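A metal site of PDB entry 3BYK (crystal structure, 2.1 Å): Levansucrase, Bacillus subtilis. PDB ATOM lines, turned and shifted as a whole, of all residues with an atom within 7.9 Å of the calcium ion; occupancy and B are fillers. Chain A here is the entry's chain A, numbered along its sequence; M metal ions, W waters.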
ATOM      1  N   GLN A 226      21.033   7.155   3.436  1.00  0.00           N
ATOM      2  CA  GLN A 226      20.233   6.231   4.210  1.00  0.00           C
ATOM      3  C   GLN A 226      18.947   5.858   3.475  1.00  0.00           C
ATOM      4  O   GLN A 226      18.320   6.720   2.871  1.00  0.00           O
ATOM      5  CB  GLN A 226      19.878   6.862   5.569  1.00  0.00           C
ATOM      6  CG  GLN A 226      19.322   5.886   6.590  1.00  0.00           C
ATOM      7  CD  GLN A 226      18.849   6.554   7.886  1.00  0.00           C
ATOM      8  OE1 GLN A 226      18.088   7.536   7.845  1.00  0.00           O
ATOM      9  NE2 GLN A 226      19.277   6.015   9.015  1.00  0.00           N
ATOM     10  N   PHE A 231      16.551   2.771   8.648  1.00  0.00           N
ATOM     11  CA  PHE A 231      15.720   3.387   9.686  1.00  0.00           C
ATOM     12  C   PHE A 231      15.009   2.311  10.498  1.00  0.00           C
ATOM     13  O   PHE A 231      14.985   2.353  11.735  1.00  0.00           O
ATOM     14  CB  PHE A 231      14.715   4.325   9.019  1.00  0.00           C
ATOM     15  CG  PHE A 231      13.783   5.029   9.959  1.00  0.00           C
ATOM     16  CD1 PHE A 231      14.259   5.816  10.984  1.00  0.00           C
ATOM     17  CD2 PHE A 231      12.403   4.947   9.766  1.00  0.00           C
ATOM     18  CE1 PHE A 231      13.375   6.503  11.830  1.00  0.00           C
ATOM     19  CE2 PHE A 231      11.525   5.622  10.579  1.00  0.00           C
ATOM     20  CZ  PHE A 231      12.008   6.398  11.631  1.00  0.00           C
ATOM     21  N   GLU A 234      17.067   0.378  13.126  1.00  0.00           N
ATOM     22  CA  GLU A 234      17.270   1.096  14.409  1.00  0.00           C
ATOM     23  C   GLU A 234      16.093   0.953  15.388  1.00  0.00           C
ATOM     24  O   GLU A 234      16.258   1.184  16.588  1.00  0.00           O
ATOM     25  CB  GLU A 234      17.491   2.595  14.169  1.00  0.00           C
ATOM     26  CG  GLU A 234      18.648   2.987  13.258  1.00  0.00           C
ATOM     27  CD  GLU A 234      20.020   2.827  13.893  1.00  0.00           C
ATOM     28  OE1 GLU A 234      20.092   2.584  15.126  1.00  0.00           O
ATOM     29  OE2 GLU A 234      21.033   2.952  13.159  1.00  0.00           O
ATOM     30  N   GLY A 240      14.425   7.272  18.048  1.00  0.00           N
ATOM     31  CA  GLY A 240      14.873   8.663  18.015  1.00  0.00           C
ATOM     32  C   GLY A 240      15.548   9.066  16.705  1.00  0.00           C
ATOM     33  O   GLY A 240      15.849  10.244  16.475  1.00  0.00           O
ATOM     34  N   ASP A 241      15.791   8.097  15.827  1.00  0.00           N
ATOM     35  CA  ASP A 241      16.360   8.398  14.511  1.00  0.00           C
ATOM     36  C   ASP A 241      15.291   9.108  13.681  1.00  0.00           C
ATOM     37  O   ASP A 241      14.109   8.997  13.962  1.00  0.00           O
ATOM     38  CB  ASP A 241      16.824   7.114  13.804  1.00  0.00           C
ATOM     39  CG  ASP A 241      17.810   7.380  12.665  1.00  0.00           C
ATOM     40  OD1 ASP A 241      18.396   8.488  12.612  1.00  0.00           O
ATOM     41  OD2 ASP A 241      18.067   6.539  11.762  1.00  0.00           O
ATOM     42  N   ASN A 242      15.726   9.854  12.680  1.00  0.00           N
ATOM     43  CA  ASN A 242      14.824  10.631  11.858  1.00  0.00           C
ATOM     44  C   ASN A 242      15.288  10.495  10.412  1.00  0.00           C
ATOM     45  O   ASN A 242      16.229  11.156   9.988  1.00  0.00           O
ATOM     46  CB  ASN A 242      14.818  12.098  12.329  1.00  0.00           C
ATOM     47  CG  ASN A 242      13.981  13.012  11.455  1.00  0.00           C
ATOM     48  OD1 ASN A 242      13.221  12.559  10.593  1.00  0.00           O
ATOM     49  ND2 ASN A 242      14.106  14.321  11.694  1.00  0.00           N
ATOM     50  N   HIS A 243      14.601   9.619   9.689  1.00  0.00           N
ATOM     51  CA  HIS A 243      14.920   9.312   8.302  1.00  0.00           C
ATOM     52  C   HIS A 243      14.272  10.298   7.337  1.00  0.00           C
ATOM     53  O   HIS A 243      13.064  10.585   7.420  1.00  0.00           O
ATOM     54  CB  HIS A 243      14.477   7.899   7.959  1.00  0.00           C
ATOM     55  CG  HIS A 243      14.624   7.568   6.509  1.00  0.00           C
ATOM     56  ND1 HIS A 243      15.837   7.271   5.940  1.00  0.00           N
ATOM     57  CD2 HIS A 243      13.719   7.519   5.502  1.00  0.00           C
ATOM     58  CE1 HIS A 243      15.671   7.021   4.657  1.00  0.00           C
ATOM     59  NE2 HIS A 243      14.390   7.164   4.365  1.00  0.00           N
ATOM     60  N   THR A 244      15.088  10.794   6.418  1.00  0.00           N
ATOM     61  CA  THR A 244      14.653  11.786   5.446  1.00  0.00           C
ATOM     62  C   THR A 244      15.208  11.417   4.076  1.00  0.00           C
ATOM     63  O   THR A 244      16.332  10.917   3.954  1.00  0.00           O
ATOM     64  CB  THR A 244      15.091  13.235   5.829  1.00  0.00           C
ATOM     65  OG1 THR A 244      16.471  13.440   5.547  1.00  0.00           O
ATOM     66  CG2 THR A 244      14.948  13.508   7.323  1.00  0.00           C
ATOM     67  N   ALA A 263      18.567  14.510   2.637  1.00  0.00           N
ATOM     68  CA  ALA A 263      18.812  13.102   2.915  1.00  0.00           C
ATOM     69  C   ALA A 263      19.505  12.938   4.263  1.00  0.00           C
ATOM     70  O   ALA A 263      19.580  13.879   5.060  1.00  0.00           O
ATOM     71  CB  ALA A 263      19.635  12.469   1.802  1.00  0.00           C
ATOM     72  N   ASN A 264      19.961  11.725   4.524  1.00  0.00           N
ATOM     73  CA  ASN A 264      20.880  11.445   5.599  1.00  0.00           C
ATOM     74  C   ASN A 264      22.011  10.618   5.024  1.00  0.00           C
ATOM     75  O   ASN A 264      21.819   9.953   4.000  1.00  0.00           O
ATOM     76  CB  ASN A 264      20.162  10.686   6.718  1.00  0.00           C
ATOM     77  CG  ASN A 264      19.016  11.500   7.313  1.00  0.00           C
ATOM     78  OD1 ASN A 264      17.884  11.416   6.837  1.00  0.00           O
ATOM     79  ND2 ASN A 264      19.301  12.283   8.352  1.00  0.00           N
ATOM     80  N   THR A 265      23.190  10.647   5.648  1.00  0.00           N
ATOM     81  CA  THR A 265      24.333   9.907   5.138  1.00  0.00           C
ATOM     82  C   THR A 265      24.126   8.415   5.255  1.00  0.00           C
ATOM     83  O   THR A 265      23.263   7.969   6.013  1.00  0.00           O
ATOM     84  CB  THR A 265      25.632  10.275   5.890  1.00  0.00           C
ATOM     85  OG1 THR A 265      25.491  10.019   7.284  1.00  0.00           O
ATOM     86  CG2 THR A 265      25.945  11.763   5.779  1.00  0.00           C
ATOM     87  N   TYR A 271      28.506   7.782   8.643  1.00  0.00           N
ATOM     88  CA  TYR A 271      27.186   7.406   9.138  1.00  0.00           C
ATOM     89  C   TYR A 271      26.977   7.869  10.586  1.00  0.00           C
ATOM     90  O   TYR A 271      27.939   8.161  11.306  1.00  0.00           O
ATOM     91  CB  TYR A 271      27.020   5.880   9.055  1.00  0.00           C
ATOM     92  CG  TYR A 271      25.585   5.366   9.069  1.00  0.00           C
ATOM     93  CD1 TYR A 271      24.604   6.008   8.329  1.00  0.00           C
ATOM     94  CD2 TYR A 271      25.238   4.228   9.805  1.00  0.00           C
ATOM     95  CE1 TYR A 271      23.284   5.533   8.326  1.00  0.00           C
ATOM     96  CE2 TYR A 271      23.912   3.756   9.808  1.00  0.00           C
ATOM     97  CZ  TYR A 271      22.947   4.426   9.058  1.00  0.00           C
ATOM     98  OH  TYR A 271      21.638   3.999   9.013  1.00  0.00           O
ATOM     99  N   GLN A 272      25.705   7.911  10.978  1.00  0.00           N
ATOM    100  CA  GLN A 272      25.331   8.015  12.381  1.00  0.00           C
ATOM    101  C   GLN A 272      25.954   6.853  13.185  1.00  0.00           C
ATOM    102  O   GLN A 272      26.299   5.822  12.622  1.00  0.00           O
ATOM    103  CB  GLN A 272      23.806   7.982  12.529  1.00  0.00           C
ATOM    104  CG  GLN A 272      23.147   6.642  12.141  1.00  0.00           C
ATOM    105  CD  GLN A 272      21.653   6.769  11.860  1.00  0.00           C
ATOM    106  OE1 GLN A 272      21.200   7.804  11.377  1.00  0.00           O
ATOM    107  NE2 GLN A 272      20.907   5.710  12.163  1.00  0.00           N
ATOM    108  N   GLY A 273      26.075   7.064  14.499  1.00  0.00           N
ATOM    109  CA  GLY A 273      26.639   6.082  15.404  1.00  0.00           C
ATOM    110  C   GLY A 273      27.446   6.731  16.517  1.00  0.00           C
ATOM    111  O   GLY A 273      27.692   7.944  16.517  1.00  0.00           O
ATOM    112  N   THR A 305      21.090  12.154  20.647  1.00  0.00           N
ATOM    113  CA  THR A 305      20.585  12.941  19.541  1.00  0.00           C
ATOM    114  C   THR A 305      21.713  13.213  18.532  1.00  0.00           C
ATOM    115  O   THR A 305      21.551  13.030  17.314  1.00  0.00           O
ATOM    116  CB  THR A 305      19.967  14.255  20.075  1.00  0.00           C
ATOM    117  OG1 THR A 305      18.816  13.955  20.862  1.00  0.00           O
ATOM    118  CG2 THR A 305      19.425  15.134  18.952  1.00  0.00           C
ATOM    119  N   ALA A 306      22.873  13.625  19.060  1.00  0.00           N
ATOM    120  CA  ALA A 306      24.040  13.942  18.236  1.00  0.00           C
ATOM    121  C   ALA A 306      24.514  12.716  17.455  1.00  0.00           C
ATOM    122  O   ALA A 306      24.816  12.818  16.279  1.00  0.00           O
ATOM    123  CB  ALA A 306      25.158  14.476  19.090  1.00  0.00           C
ATOM    124  N   GLU A 307      24.550  11.573  18.123  1.00  0.00           N
ATOM    125  CA  GLU A 307      24.988  10.325  17.509  1.00  0.00           C
ATOM    126  C   GLU A 307      24.106   9.970  16.312  1.00  0.00           C
ATOM    127  O   GLU A 307      24.603   9.561  15.259  1.00  0.00           O
ATOM    128  CB  GLU A 307      25.011   9.192  18.550  1.00  0.00           C
ATOM    129  CG  GLU A 307      26.195   9.297  19.523  1.00  0.00           C
ATOM    130  CD  GLU A 307      26.064   8.421  20.745  1.00  0.00           C
ATOM    131  OE1 GLU A 307      24.953   7.987  21.060  1.00  0.00           O
ATOM    132  OE2 GLU A 307      27.097   8.153  21.406  1.00  0.00           O
ATOM    133  N   LEU A 308      22.796  10.194  16.466  1.00  0.00           N
ATOM    134  CA  LEU A 308      21.813   9.910  15.418  1.00  0.00           C
ATOM    135  C   LEU A 308      21.764  10.966  14.308  1.00  0.00           C
ATOM    136  O   LEU A 308      21.223  10.721  13.235  1.00  0.00           O
ATOM    137  CB  LEU A 308      20.413   9.829  16.033  1.00  0.00           C
ATOM    138  CG  LEU A 308      20.164   8.665  17.002  1.00  0.00           C
ATOM    139  CD1 LEU A 308      18.921   8.929  17.825  1.00  0.00           C
ATOM    140  CD2 LEU A 308      20.039   7.369  16.246  1.00  0.00           C
ATOM    141  N   ALA A 309      22.320  12.144  14.584  1.00  0.00           N
ATOM    142  CA  ALA A 309      22.261  13.264  13.646  1.00  0.00           C
ATOM    143  C   ALA A 309      23.232  13.072  12.479  1.00  0.00           C
ATOM    144  O   ALA A 309      24.445  13.091  12.676  1.00  0.00           O
ATOM    145  CB  ALA A 309      22.549  14.553  14.378  1.00  0.00           C
ATOM    146  N   ASN A 310      22.699  12.856  11.283  1.00  0.00           N
ATOM    147  CA  ASN A 310      23.523  12.684  10.090  1.00  0.00           C
ATOM    148  C   ASN A 310      22.823  13.195   8.842  1.00  0.00           C
ATOM    149  O   ASN A 310      22.787  12.530   7.814  1.00  0.00           O
ATOM    150  CB  ASN A 310      23.991  11.224   9.945  1.00  0.00           C
ATOM    151  CG  ASN A 310      22.869  10.287   9.533  1.00  0.00           C
ATOM    152  OD1 ASN A 310      21.714  10.508   9.880  1.00  0.00           O
ATOM    153  ND2 ASN A 310      23.220   9.242   8.786  1.00  0.00           N
ATOM    154  N   GLY A 311      22.283  14.404   8.930  1.00  0.00           N
ATOM    155  CA  GLY A 311      21.635  15.056   7.810  1.00  0.00           C
ATOM    156  C   GLY A 311      22.613  15.319   6.694  1.00  0.00           C
ATOM    157  O   GLY A 311      23.831  15.423   6.919  1.00  0.00           O
ATOM    158  N   THR A 338      22.484  18.073  13.461  1.00  0.00           N
ATOM    159  CA  THR A 338      21.089  17.742  13.256  1.00  0.00           C
ATOM    160  C   THR A 338      20.921  16.676  12.190  1.00  0.00           C
ATOM    161  O   THR A 338      21.754  16.529  11.297  1.00  0.00           O
ATOM    162  CB  THR A 338      20.288  18.997  12.874  1.00  0.00           C
ATOM    163  OG1 THR A 338      18.907  18.670  12.682  1.00  0.00           O
ATOM    164  CG2 THR A 338      20.754  19.566  11.545  1.00  0.00           C
ATOM    165  N   ASP A 339      19.813  15.948  12.319  1.00  0.00           N
ATOM    166  CA  ASP A 339      19.358  14.937  11.384  1.00  0.00           C
ATOM    167  C   ASP A 339      18.471  15.502  10.278  1.00  0.00           C
ATOM    168  O   ASP A 339      18.077  14.775   9.342  1.00  0.00           O
ATOM    169  CB  ASP A 339      18.516  13.909  12.159  1.00  0.00           C
ATOM    170  CG  ASP A 339      18.936  12.481  11.921  1.00  0.00           C
ATOM    171  OD1 ASP A 339      19.812  12.231  11.072  1.00  0.00           O
ATOM    172  OD2 ASP A 339      18.417  11.537  12.544  1.00  0.00           O
ATOM    173  N   GLU A 340      18.127  16.791  10.385  1.00  0.00           N
ATOM    174  CA  GLU A 340      17.064  17.369   9.573  1.00  0.00           C
ATOM    175  C   GLU A 340      17.424  18.720   8.984  1.00  0.00           C
ATOM    176  O   GLU A 340      17.200  19.774   9.604  1.00  0.00           O
ATOM    177  CB  GLU A 340      15.781  17.451  10.389  1.00  0.00           C
ATOM    178  CG  GLU A 340      14.544  17.741   9.551  1.00  0.00           C
ATOM    179  CD  GLU A 340      13.277  17.749  10.401  1.00  0.00           C
ATOM    180  OE1 GLU A 340      12.679  16.681  10.560  1.00  0.00           O
ATOM    181  OE2 GLU A 340      12.921  18.832  10.931  1.00  0.00           O
HETATM  182 CA    CA M   1      19.951   9.811  11.484  1.00  0.00          CA
HETATM  183  O   HOH W   1      18.436   9.534   9.581  1.00  0.00           O
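Water W1 lies within hydrogen-bond range of OE1 of Gln 226 (2.7 Å), O of Asn 242 (2.8 Å) and ND2 of Asn 264 (3.1 Å).
OD2 of Asp 339 lies close to N of Asn 242.
O of Asp 339 sits at hydrogen-bond distance from ND2 of Asn 264 (2.9 Å).
OD2 of Asp 241 lies within hydrogen-bond range of NE2 of Gln 226.
NE2 of Gln 272 lies within hydrogen-bond range of OE2 of Glu 234 (2.9 Å).
The side-chain amide oxygen of Asn 310 sits close to the side-chain amide nitrogen of Asn 264 (3.4 Å).
ND2 of Asn 310 is in hydrogen-bond range of OG1 of Thr 265.
OD1 of Asp 241 binds the calcium ion (2.3 Å).
The calcium ion is bound by O of Leu 308, 2.3 Å away.
OE1 of Gln 272 binds the calcium ion, at 2.4 Å.
The calcium ion is bound by water W1 (2.4 Å).
The calcium ion is bound by OD1 of Asp 339 (2.5 Å).
OD1 of Asn 310 is bound to the calcium ion, 2.5 Å away.
The calcium ion is bound by OD2 of Asp 339 (2.5 Å).
The calcium ion has seven donor atoms within binding distance.
Of the 24 residues printed, 5 come within 4 Å of the calcium ion.
Along chain A the residues within 4 Å of the calcium ion span positions 241 to 339.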
